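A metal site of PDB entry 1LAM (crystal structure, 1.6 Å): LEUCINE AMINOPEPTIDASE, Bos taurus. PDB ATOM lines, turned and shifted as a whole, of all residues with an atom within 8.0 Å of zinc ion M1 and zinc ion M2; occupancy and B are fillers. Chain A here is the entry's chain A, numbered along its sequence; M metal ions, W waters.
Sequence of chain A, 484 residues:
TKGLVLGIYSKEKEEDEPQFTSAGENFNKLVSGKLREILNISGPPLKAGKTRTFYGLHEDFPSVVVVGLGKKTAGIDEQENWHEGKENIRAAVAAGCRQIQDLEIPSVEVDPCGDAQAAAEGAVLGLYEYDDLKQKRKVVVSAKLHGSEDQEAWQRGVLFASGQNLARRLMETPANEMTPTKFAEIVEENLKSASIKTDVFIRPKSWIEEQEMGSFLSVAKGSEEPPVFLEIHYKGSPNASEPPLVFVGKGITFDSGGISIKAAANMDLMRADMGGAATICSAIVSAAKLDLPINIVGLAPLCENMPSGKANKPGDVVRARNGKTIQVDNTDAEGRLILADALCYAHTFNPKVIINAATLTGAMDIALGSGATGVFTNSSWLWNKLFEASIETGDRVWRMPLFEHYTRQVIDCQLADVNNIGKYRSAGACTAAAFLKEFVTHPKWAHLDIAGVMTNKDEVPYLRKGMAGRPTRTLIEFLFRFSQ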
ATOM      1  N   VAL A 219      -2.702 -19.489 -15.093  1.00  0.00           N
ATOM      2  CA  VAL A 219      -1.871 -20.598 -15.525  1.00  0.00           C
ATOM      3  C   VAL A 219      -2.284 -21.058 -16.924  1.00  0.00           C
ATOM      4  O   VAL A 219      -1.441 -21.224 -17.809  1.00  0.00           O
ATOM      5  CB  VAL A 219      -2.004 -21.790 -14.558  1.00  0.00           C
ATOM      6  CG1 VAL A 219      -1.233 -22.994 -15.086  1.00  0.00           C
ATOM      7  CG2 VAL A 219      -1.496 -21.400 -13.178  1.00  0.00           C
ATOM      8  N   LYS A 250      -4.888 -31.855  -8.802  1.00  0.00           N
ATOM      9  CA  LYS A 250      -4.161 -30.979  -9.725  1.00  0.00           C
ATOM     10  C   LYS A 250      -4.160 -31.634 -11.113  1.00  0.00           C
ATOM     11  O   LYS A 250      -3.621 -32.744 -11.279  1.00  0.00           O
ATOM     12  CB  LYS A 250      -2.713 -30.809  -9.238  1.00  0.00           C
ATOM     13  CG  LYS A 250      -1.792 -30.100 -10.236  1.00  0.00           C
ATOM     14  CD  LYS A 250      -0.346 -30.078  -9.747  1.00  0.00           C
ATOM     15  CE  LYS A 250       0.594 -29.600 -10.864  1.00  0.00           C
ATOM     16  NZ  LYS A 250       2.031 -29.568 -10.458  1.00  0.00           N
ATOM     17  N   GLY A 251      -4.760 -30.957 -12.090  1.00  0.00           N
ATOM     18  CA  GLY A 251      -4.821 -31.490 -13.449  1.00  0.00           C
ATOM     19  C   GLY A 251      -4.038 -30.750 -14.522  1.00  0.00           C
ATOM     20  O   GLY A 251      -4.611 -30.279 -15.517  1.00  0.00           O
ATOM     21  N   ILE A 252      -2.729 -30.604 -14.346  1.00  0.00           N
ATOM     22  CA  ILE A 252      -1.906 -29.947 -15.349  1.00  0.00           C
ATOM     23  C   ILE A 252      -1.586 -31.071 -16.356  1.00  0.00           C
ATOM     24  O   ILE A 252      -0.777 -31.958 -16.077  1.00  0.00           O
ATOM     25  CB  ILE A 252      -0.623 -29.354 -14.715  1.00  0.00           C
ATOM     26  CG1 ILE A 252      -0.990 -28.204 -13.757  1.00  0.00           C
ATOM     27  CG2 ILE A 252       0.333 -28.856 -15.808  1.00  0.00           C
ATOM     28  CD1 ILE A 252      -1.569 -26.946 -14.443  1.00  0.00           C
ATOM     29  N   THR A 253      -2.252 -31.057 -17.511  1.00  0.00           N
ATOM     30  CA  THR A 253      -2.066 -32.111 -18.517  1.00  0.00           C
ATOM     31  C   THR A 253      -0.653 -32.173 -19.103  1.00  0.00           C
ATOM     32  O   THR A 253      -0.212 -33.220 -19.597  1.00  0.00           O
ATOM     33  CB  THR A 253      -3.187 -32.078 -19.586  1.00  0.00           C
ATOM     34  OG1 THR A 253      -3.224 -30.792 -20.213  1.00  0.00           O
ATOM     35  CG2 THR A 253      -4.541 -32.328 -18.927  1.00  0.00           C
ATOM     36  N   PHE A 254       0.020 -31.025 -19.109  1.00  0.00           N
ATOM     37  CA  PHE A 254       1.428 -30.932 -19.496  1.00  0.00           C
ATOM     38  C   PHE A 254       2.026 -29.680 -18.866  1.00  0.00           C
ATOM     39  O   PHE A 254       1.455 -28.587 -18.964  1.00  0.00           O
ATOM     40  CB  PHE A 254       1.747 -30.932 -20.996  1.00  0.00           C
ATOM     41  CG  PHE A 254       3.243 -31.043 -21.259  1.00  0.00           C
ATOM     42  CD1 PHE A 254       3.878 -32.280 -21.104  1.00  0.00           C
ATOM     43  CD2 PHE A 254       4.024 -29.909 -21.475  1.00  0.00           C
ATOM     44  CE1 PHE A 254       5.277 -32.378 -21.176  1.00  0.00           C
ATOM     45  CE2 PHE A 254       5.415 -30.005 -21.551  1.00  0.00           C
ATOM     46  CZ  PHE A 254       6.044 -31.236 -21.385  1.00  0.00           C
ATOM     47  N   ASP A 255       3.163 -29.872 -18.220  1.00  0.00           N
ATOM     48  CA  ASP A 255       3.860 -28.783 -17.543  1.00  0.00           C
ATOM     49  C   ASP A 255       5.261 -28.559 -18.154  1.00  0.00           C
ATOM     50  O   ASP A 255       6.178 -29.373 -17.931  1.00  0.00           O
ATOM     51  CB  ASP A 255       3.977 -29.116 -16.048  1.00  0.00           C
ATOM     52  CG  ASP A 255       4.509 -27.967 -15.221  1.00  0.00           C
ATOM     53  OD1 ASP A 255       4.588 -26.831 -15.740  1.00  0.00           O
ATOM     54  OD2 ASP A 255       4.851 -28.216 -14.040  1.00  0.00           O
ATOM     55  N   SER A 256       5.418 -27.477 -18.915  1.00  0.00           N
ATOM     56  CA  SER A 256       6.713 -27.120 -19.496  1.00  0.00           C
ATOM     57  C   SER A 256       7.463 -26.205 -18.515  1.00  0.00           C
ATOM     58  O   SER A 256       8.650 -25.883 -18.708  1.00  0.00           O
ATOM     59  CB  SER A 256       6.523 -26.334 -20.798  1.00  0.00           C
ATOM     60  OG  SER A 256       6.034 -25.030 -20.507  1.00  0.00           O
ATOM     61  N   GLY A 257       6.738 -25.763 -17.492  1.00  0.00           N
ATOM     62  CA  GLY A 257       7.274 -24.860 -16.503  1.00  0.00           C
ATOM     63  C   GLY A 257       6.834 -23.428 -16.816  1.00  0.00           C
ATOM     64  O   GLY A 257       6.762 -22.590 -15.919  1.00  0.00           O
ATOM     65  N   GLY A 258       6.469 -23.179 -18.082  1.00  0.00           N
ATOM     66  CA  GLY A 258       6.066 -21.844 -18.512  1.00  0.00           C
ATOM     67  C   GLY A 258       7.292 -20.986 -18.777  1.00  0.00           C
ATOM     68  O   GLY A 258       8.319 -21.500 -19.227  1.00  0.00           O
ATOM     69  N   SER A 260       9.260 -19.774 -16.645  1.00  0.00           N
ATOM     70  CA  SER A 260      10.288 -20.333 -15.755  1.00  0.00           C
ATOM     71  C   SER A 260      10.426 -21.758 -16.296  1.00  0.00           C
ATOM     72  O   SER A 260      10.182 -22.747 -15.580  1.00  0.00           O
ATOM     73  CB  SER A 260       9.744 -20.371 -14.325  1.00  0.00           C
ATOM     74  OG  SER A 260       9.418 -19.079 -13.848  1.00  0.00           O
ATOM     75  N   LYS A 262      11.303 -25.463 -17.811  1.00  0.00           N
ATOM     76  CA  LYS A 262      12.016 -26.639 -17.306  1.00  0.00           C
ATOM     77  C   LYS A 262      13.194 -27.045 -18.197  1.00  0.00           C
ATOM     78  O   LYS A 262      13.290 -26.626 -19.350  1.00  0.00           O
ATOM     79  CB  LYS A 262      11.068 -27.841 -17.213  1.00  0.00           C
ATOM     80  CG  LYS A 262      10.005 -27.714 -16.162  1.00  0.00           C
ATOM     81  CD  LYS A 262       9.086 -28.949 -16.198  1.00  0.00           C
ATOM     82  CE  LYS A 262       8.063 -28.923 -15.087  1.00  0.00           C
ATOM     83  NZ  LYS A 262       8.710 -28.922 -13.748  1.00  0.00           N
ATOM     84  N   MET A 270       6.352 -35.028 -17.635  1.00  0.00           N
ATOM     85  CA  MET A 270       5.423 -33.997 -17.182  1.00  0.00           C
ATOM     86  C   MET A 270       4.017 -34.149 -17.790  1.00  0.00           C
ATOM     87  O   MET A 270       3.103 -33.368 -17.483  1.00  0.00           O
ATOM     88  CB  MET A 270       6.003 -32.598 -17.400  1.00  0.00           C
ATOM     89  CG  MET A 270       7.209 -32.297 -16.513  1.00  0.00           C
ATOM     90  SD  MET A 270       6.788 -32.459 -14.727  1.00  0.00           S
ATOM     91  CE  MET A 270       7.498 -34.003 -14.362  1.00  0.00           C
ATOM     92  N   ALA A 272       2.408 -36.417 -17.013  1.00  0.00           N
ATOM     93  CA  ALA A 272       1.744 -36.985 -15.841  1.00  0.00           C
ATOM     94  C   ALA A 272       1.561 -35.971 -14.718  1.00  0.00           C
ATOM     95  O   ALA A 272       1.266 -36.367 -13.583  1.00  0.00           O
ATOM     96  CB  ALA A 272       2.498 -38.219 -15.335  1.00  0.00           C
ATOM     97  N   ASP A 273       1.693 -34.682 -15.036  1.00  0.00           N
ATOM     98  CA  ASP A 273       1.526 -33.640 -14.009  1.00  0.00           C
ATOM     99  C   ASP A 273       0.037 -33.489 -13.652  1.00  0.00           C
ATOM    100  O   ASP A 273      -0.348 -32.588 -12.906  1.00  0.00           O
ATOM    101  CB  ASP A 273       2.133 -32.314 -14.476  1.00  0.00           C
ATOM    102  CG  ASP A 273       2.594 -31.425 -13.308  1.00  0.00           C
ATOM    103  OD1 ASP A 273       2.969 -31.930 -12.222  1.00  0.00           O
ATOM    104  OD2 ASP A 273       2.609 -30.182 -13.494  1.00  0.00           O
ATOM    105  N   MET A 274      -0.799 -34.354 -14.236  1.00  0.00           N
ATOM    106  CA  MET A 274      -2.222 -34.382 -13.949  1.00  0.00           C
ATOM    107  C   MET A 274      -2.522 -35.634 -13.100  1.00  0.00           C
ATOM    108  O   MET A 274      -3.685 -36.034 -12.971  1.00  0.00           O
ATOM    109  CB  MET A 274      -3.051 -34.365 -15.254  1.00  0.00           C
ATOM    110  CG  MET A 274      -2.445 -35.143 -16.448  1.00  0.00           C
ATOM    111  SD  MET A 274      -2.141 -36.895 -16.147  1.00  0.00           S
ATOM    112  CE  MET A 274      -3.818 -37.520 -16.050  1.00  0.00           C
ATOM    113  N   ASN A 305       0.521 -25.794 -18.946  1.00  0.00           N
ATOM    114  CA  ASN A 305       1.374 -24.694 -18.485  1.00  0.00           C
ATOM    115  C   ASN A 305       2.422 -24.573 -19.596  1.00  0.00           C
ATOM    116  O   ASN A 305       3.380 -25.352 -19.651  1.00  0.00           O
ATOM    117  CB  ASN A 305       2.035 -25.010 -17.124  1.00  0.00           C
ATOM    118  CG  ASN A 305       2.701 -23.796 -16.488  1.00  0.00           C
ATOM    119  OD1 ASN A 305       2.331 -22.652 -16.774  1.00  0.00           O
ATOM    120  ND2 ASN A 305       3.671 -24.024 -15.621  1.00  0.00           N
ATOM    121  N   ASN A 330       7.645 -17.764  -9.603  1.00  0.00           N
ATOM    122  CA  ASN A 330       8.138 -18.842 -10.468  1.00  0.00           C
ATOM    123  C   ASN A 330       6.901 -19.489 -11.108  1.00  0.00           C
ATOM    124  O   ASN A 330       6.052 -20.040 -10.410  1.00  0.00           O
ATOM    125  CB  ASN A 330       8.940 -19.845  -9.628  1.00  0.00           C
ATOM    126  CG  ASN A 330       9.580 -20.914 -10.471  1.00  0.00           C
ATOM    127  OD1 ASN A 330       8.889 -21.594 -11.216  1.00  0.00           O
ATOM    128  ND2 ASN A 330      10.899 -21.040 -10.402  1.00  0.00           N
ATOM    129  N   THR A 331       6.781 -19.380 -12.437  1.00  0.00           N
ATOM    130  CA  THR A 331       5.629 -19.917 -13.160  1.00  0.00           C
ATOM    131  C   THR A 331       5.530 -21.448 -13.175  1.00  0.00           C
ATOM    132  O   THR A 331       4.519 -22.002 -13.635  1.00  0.00           O
ATOM    133  CB  THR A 331       5.555 -19.380 -14.613  1.00  0.00           C
ATOM    134  OG1 THR A 331       6.656 -19.907 -15.380  1.00  0.00           O
ATOM    135  CG2 THR A 331       5.641 -17.850 -14.636  1.00  0.00           C
ATOM    136  N   ASP A 332       6.590 -22.122 -12.729  1.00  0.00           N
ATOM    137  CA  ASP A 332       6.611 -23.567 -12.675  1.00  0.00           C
ATOM    138  C   ASP A 332       5.982 -24.047 -11.350  1.00  0.00           C
ATOM    139  O   ASP A 332       5.785 -25.246 -11.157  1.00  0.00           O
ATOM    140  CB  ASP A 332       8.044 -24.092 -12.861  1.00  0.00           C
ATOM    141  CG  ASP A 332       8.095 -25.609 -13.162  1.00  0.00           C
ATOM    142  OD1 ASP A 332       7.036 -26.263 -13.413  1.00  0.00           O
ATOM    143  OD2 ASP A 332       9.223 -26.138 -13.161  1.00  0.00           O
ATOM    144  N   ALA A 333       5.697 -23.125 -10.434  1.00  0.00           N
ATOM    145  CA  ALA A 333       5.026 -23.481  -9.171  1.00  0.00           C
ATOM    146  C   ALA A 333       3.541 -23.181  -9.455  1.00  0.00           C
ATOM    147  O   ALA A 333       2.897 -22.378  -8.753  1.00  0.00           O
ATOM    148  CB  ALA A 333       5.553 -22.633  -8.014  1.00  0.00           C
ATOM    149  N   GLU A 334       3.037 -23.778 -10.531  1.00  0.00           N
ATOM    150  CA  GLU A 334       1.662 -23.552 -11.000  1.00  0.00           C
ATOM    151  C   GLU A 334       0.577 -24.434 -10.395  1.00  0.00           C
ATOM    152  O   GLU A 334      -0.598 -24.032 -10.348  1.00  0.00           O
ATOM    153  CB  GLU A 334       1.597 -23.632 -12.549  1.00  0.00           C
ATOM    154  CG  GLU A 334       1.355 -25.032 -13.148  1.00  0.00           C
ATOM    155  CD  GLU A 334       2.479 -26.026 -12.889  1.00  0.00           C
ATOM    156  OE1 GLU A 334       3.667 -25.624 -12.915  1.00  0.00           O
ATOM    157  OE2 GLU A 334       2.185 -27.233 -12.679  1.00  0.00           O
ATOM    158  N   GLY A 335       0.961 -25.618  -9.928  1.00  0.00           N
ATOM    159  CA  GLY A 335      -0.019 -26.513  -9.345  1.00  0.00           C
ATOM    160  C   GLY A 335      -0.702 -25.866  -8.155  1.00  0.00           C
ATOM    161  O   GLY A 335      -1.943 -25.933  -8.035  1.00  0.00           O
ATOM    162  N   ARG A 336       0.080 -25.207  -7.311  1.00  0.00           N
ATOM    163  CA  ARG A 336      -0.475 -24.557  -6.130  1.00  0.00           C
ATOM    164  C   ARG A 336      -1.397 -23.397  -6.516  1.00  0.00           C
ATOM    165  O   ARG A 336      -2.377 -23.097  -5.815  1.00  0.00           O
ATOM    166  CB  ARG A 336       0.627 -24.146  -5.129  1.00  0.00           C
ATOM    167  CG  ARG A 336       1.541 -23.009  -5.568  1.00  0.00           C
ATOM    168  CD  ARG A 336       2.807 -22.986  -4.713  1.00  0.00           C
ATOM    169  NE  ARG A 336       3.747 -24.044  -5.117  1.00  0.00           N
ATOM    170  CZ  ARG A 336       4.956 -24.239  -4.595  1.00  0.00           C
ATOM    171  NH1 ARG A 336       5.409 -23.480  -3.609  1.00  0.00           N
ATOM    172  NH2 ARG A 336       5.722 -25.230  -5.056  1.00  0.00           N
ATOM    173  N   ILE A 338      -3.484 -23.278  -9.314  1.00  0.00           N
ATOM    174  CA  ILE A 338      -4.780 -23.815  -9.712  1.00  0.00           C
ATOM    175  C   ILE A 338      -5.503 -24.477  -8.512  1.00  0.00           C
ATOM    176  O   ILE A 338      -6.745 -24.441  -8.434  1.00  0.00           O
ATOM    177  CB  ILE A 338      -4.691 -24.802 -10.947  1.00  0.00           C
ATOM    178  CG1 ILE A 338      -4.214 -26.198 -10.533  1.00  0.00           C
ATOM    179  CG2 ILE A 338      -3.763 -24.203 -12.037  1.00  0.00           C
ATOM    180  CD1 ILE A 338      -4.225 -27.202 -11.689  1.00  0.00           C
ATOM    181  N   ALA A 358      -1.739 -34.091  -5.573  1.00  0.00           N
ATOM    182  CA  ALA A 358      -1.003 -33.357  -6.590  1.00  0.00           C
ATOM    183  C   ALA A 358       0.437 -33.834  -6.760  1.00  0.00           C
ATOM    184  O   ALA A 358       1.097 -34.157  -5.769  1.00  0.00           O
ATOM    185  CB  ALA A 358      -0.982 -31.875  -6.225  1.00  0.00           C
ATOM    186  N   THR A 359       0.910 -33.868  -8.008  1.00  0.00           N
ATOM    187  CA  THR A 359       2.308 -34.213  -8.318  1.00  0.00           C
ATOM    188  C   THR A 359       2.883 -32.812  -8.158  1.00  0.00           C
ATOM    189  O   THR A 359       3.235 -32.140  -9.133  1.00  0.00           O
ATOM    190  CB  THR A 359       2.456 -34.705  -9.782  1.00  0.00           C
ATOM    191  OG1 THR A 359       1.757 -33.837 -10.668  1.00  0.00           O
ATOM    192  CG2 THR A 359       1.917 -36.124  -9.952  1.00  0.00           C
ATOM    193  N   LEU A 360       2.990 -32.370  -6.907  1.00  0.00           N
ATOM    194  CA  LEU A 360       3.401 -31.004  -6.632  1.00  0.00           C
ATOM    195  C   LEU A 360       4.848 -30.549  -6.638  1.00  0.00           C
ATOM    196  O   LEU A 360       5.166 -29.540  -7.286  1.00  0.00           O
ATOM    197  CB  LEU A 360       2.685 -30.509  -5.369  1.00  0.00           C
ATOM    198  CG  LEU A 360       2.393 -29.001  -5.257  1.00  0.00           C
ATOM    199  CD1 LEU A 360       1.399 -28.551  -6.327  1.00  0.00           C
ATOM    200  CD2 LEU A 360       1.849 -28.677  -3.870  1.00  0.00           C
ATOM    201  N   THR A 361       5.752 -31.259  -5.950  1.00  0.00           N
ATOM    202  CA  THR A 361       7.122 -30.761  -5.884  1.00  0.00           C
ATOM    203  C   THR A 361       8.234 -31.763  -6.100  1.00  0.00           C
ATOM    204  O   THR A 361       8.130 -32.928  -5.696  1.00  0.00           O
ATOM    205  CB  THR A 361       7.399 -30.075  -4.498  1.00  0.00           C
ATOM    206  OG1 THR A 361       7.358 -31.063  -3.450  1.00  0.00           O
ATOM    207  CG2 THR A 361       6.366 -28.973  -4.197  1.00  0.00           C
HETATM  208 ZN    ZN M   1       3.215 -28.876 -12.134  1.00  0.00          ZN
HETATM  209 ZN    ZN M   2       5.314 -26.751 -12.572  1.00  0.00          ZN
HETATM  210  O   HOH W   1       4.802 -28.177 -11.239  1.00  0.00           O
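Of the 29 residues printed, 4 come within 4 Å of zinc ion M1.
The nearest printed residue that does not touch zinc ion M1 is Thr 359 (4.4 Å).
Zinc ion M1 is bound by water W1, OD2 of Asp 273, OE2 of Glu 334, NZ of Lys 250 and OD2 of Asp 255.
The side-chain carboxylate (OD1) of Asp 332 is bound to zinc ion M2 (2.0 Å).
Water W1 is bound to zinc ion M2, 2.0 Å away.
Zinc ion M2 is bound by the side-chain carboxylate (OE1) of Glu 334, at 2.0 Å.
O of Asp 332 is bound to zinc ion M2 (2.1 Å).
Zinc ion M2 is bound by OD2 of Asp 255, 2.1 Å away.
Zinc ion M2 has five donor atoms within binding distance.
The side-chain amino group (NZ) of Lys 250 sits close to the backbone carbonyl oxygen (O) of Thr 359 (3.1 Å).
OD1 of Asp 255 lies within hydrogen-bond range of N of Gly 257, 3.0 Å away.
The backbone NH (N) of Asp 332 sits at hydrogen-bond distance from the side-chain amide oxygen (OD1) of Asn 330 (2.8 Å).
OE1 of Glu 334 lies close to ND2 of Asn 305, 3.1 Å away.
The backbone carbonyl oxygen (O) of Gly 257 sits at hydrogen-bond distance from the backbone NH (N) of Asp 332 (3.2 Å).
OD2 of Asp 255 lies close to NZ of Lys 262 (3.9 Å).
O of Asp 273 sits at hydrogen-bond distance from N of Ile 252, at 3.4 Å.
The side-chain carboxylate (OD2) of Asp 332 lies within salt-bridge range of the side-chain amino group (NZ) of Lys 262 (2.9 Å).
Within 4 Å of zinc ion M2: Asp 255, Asp 332 and Glu 334.
The nearest printed residue that does not touch zinc ion M2 is Lys 262 (4.2 Å).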
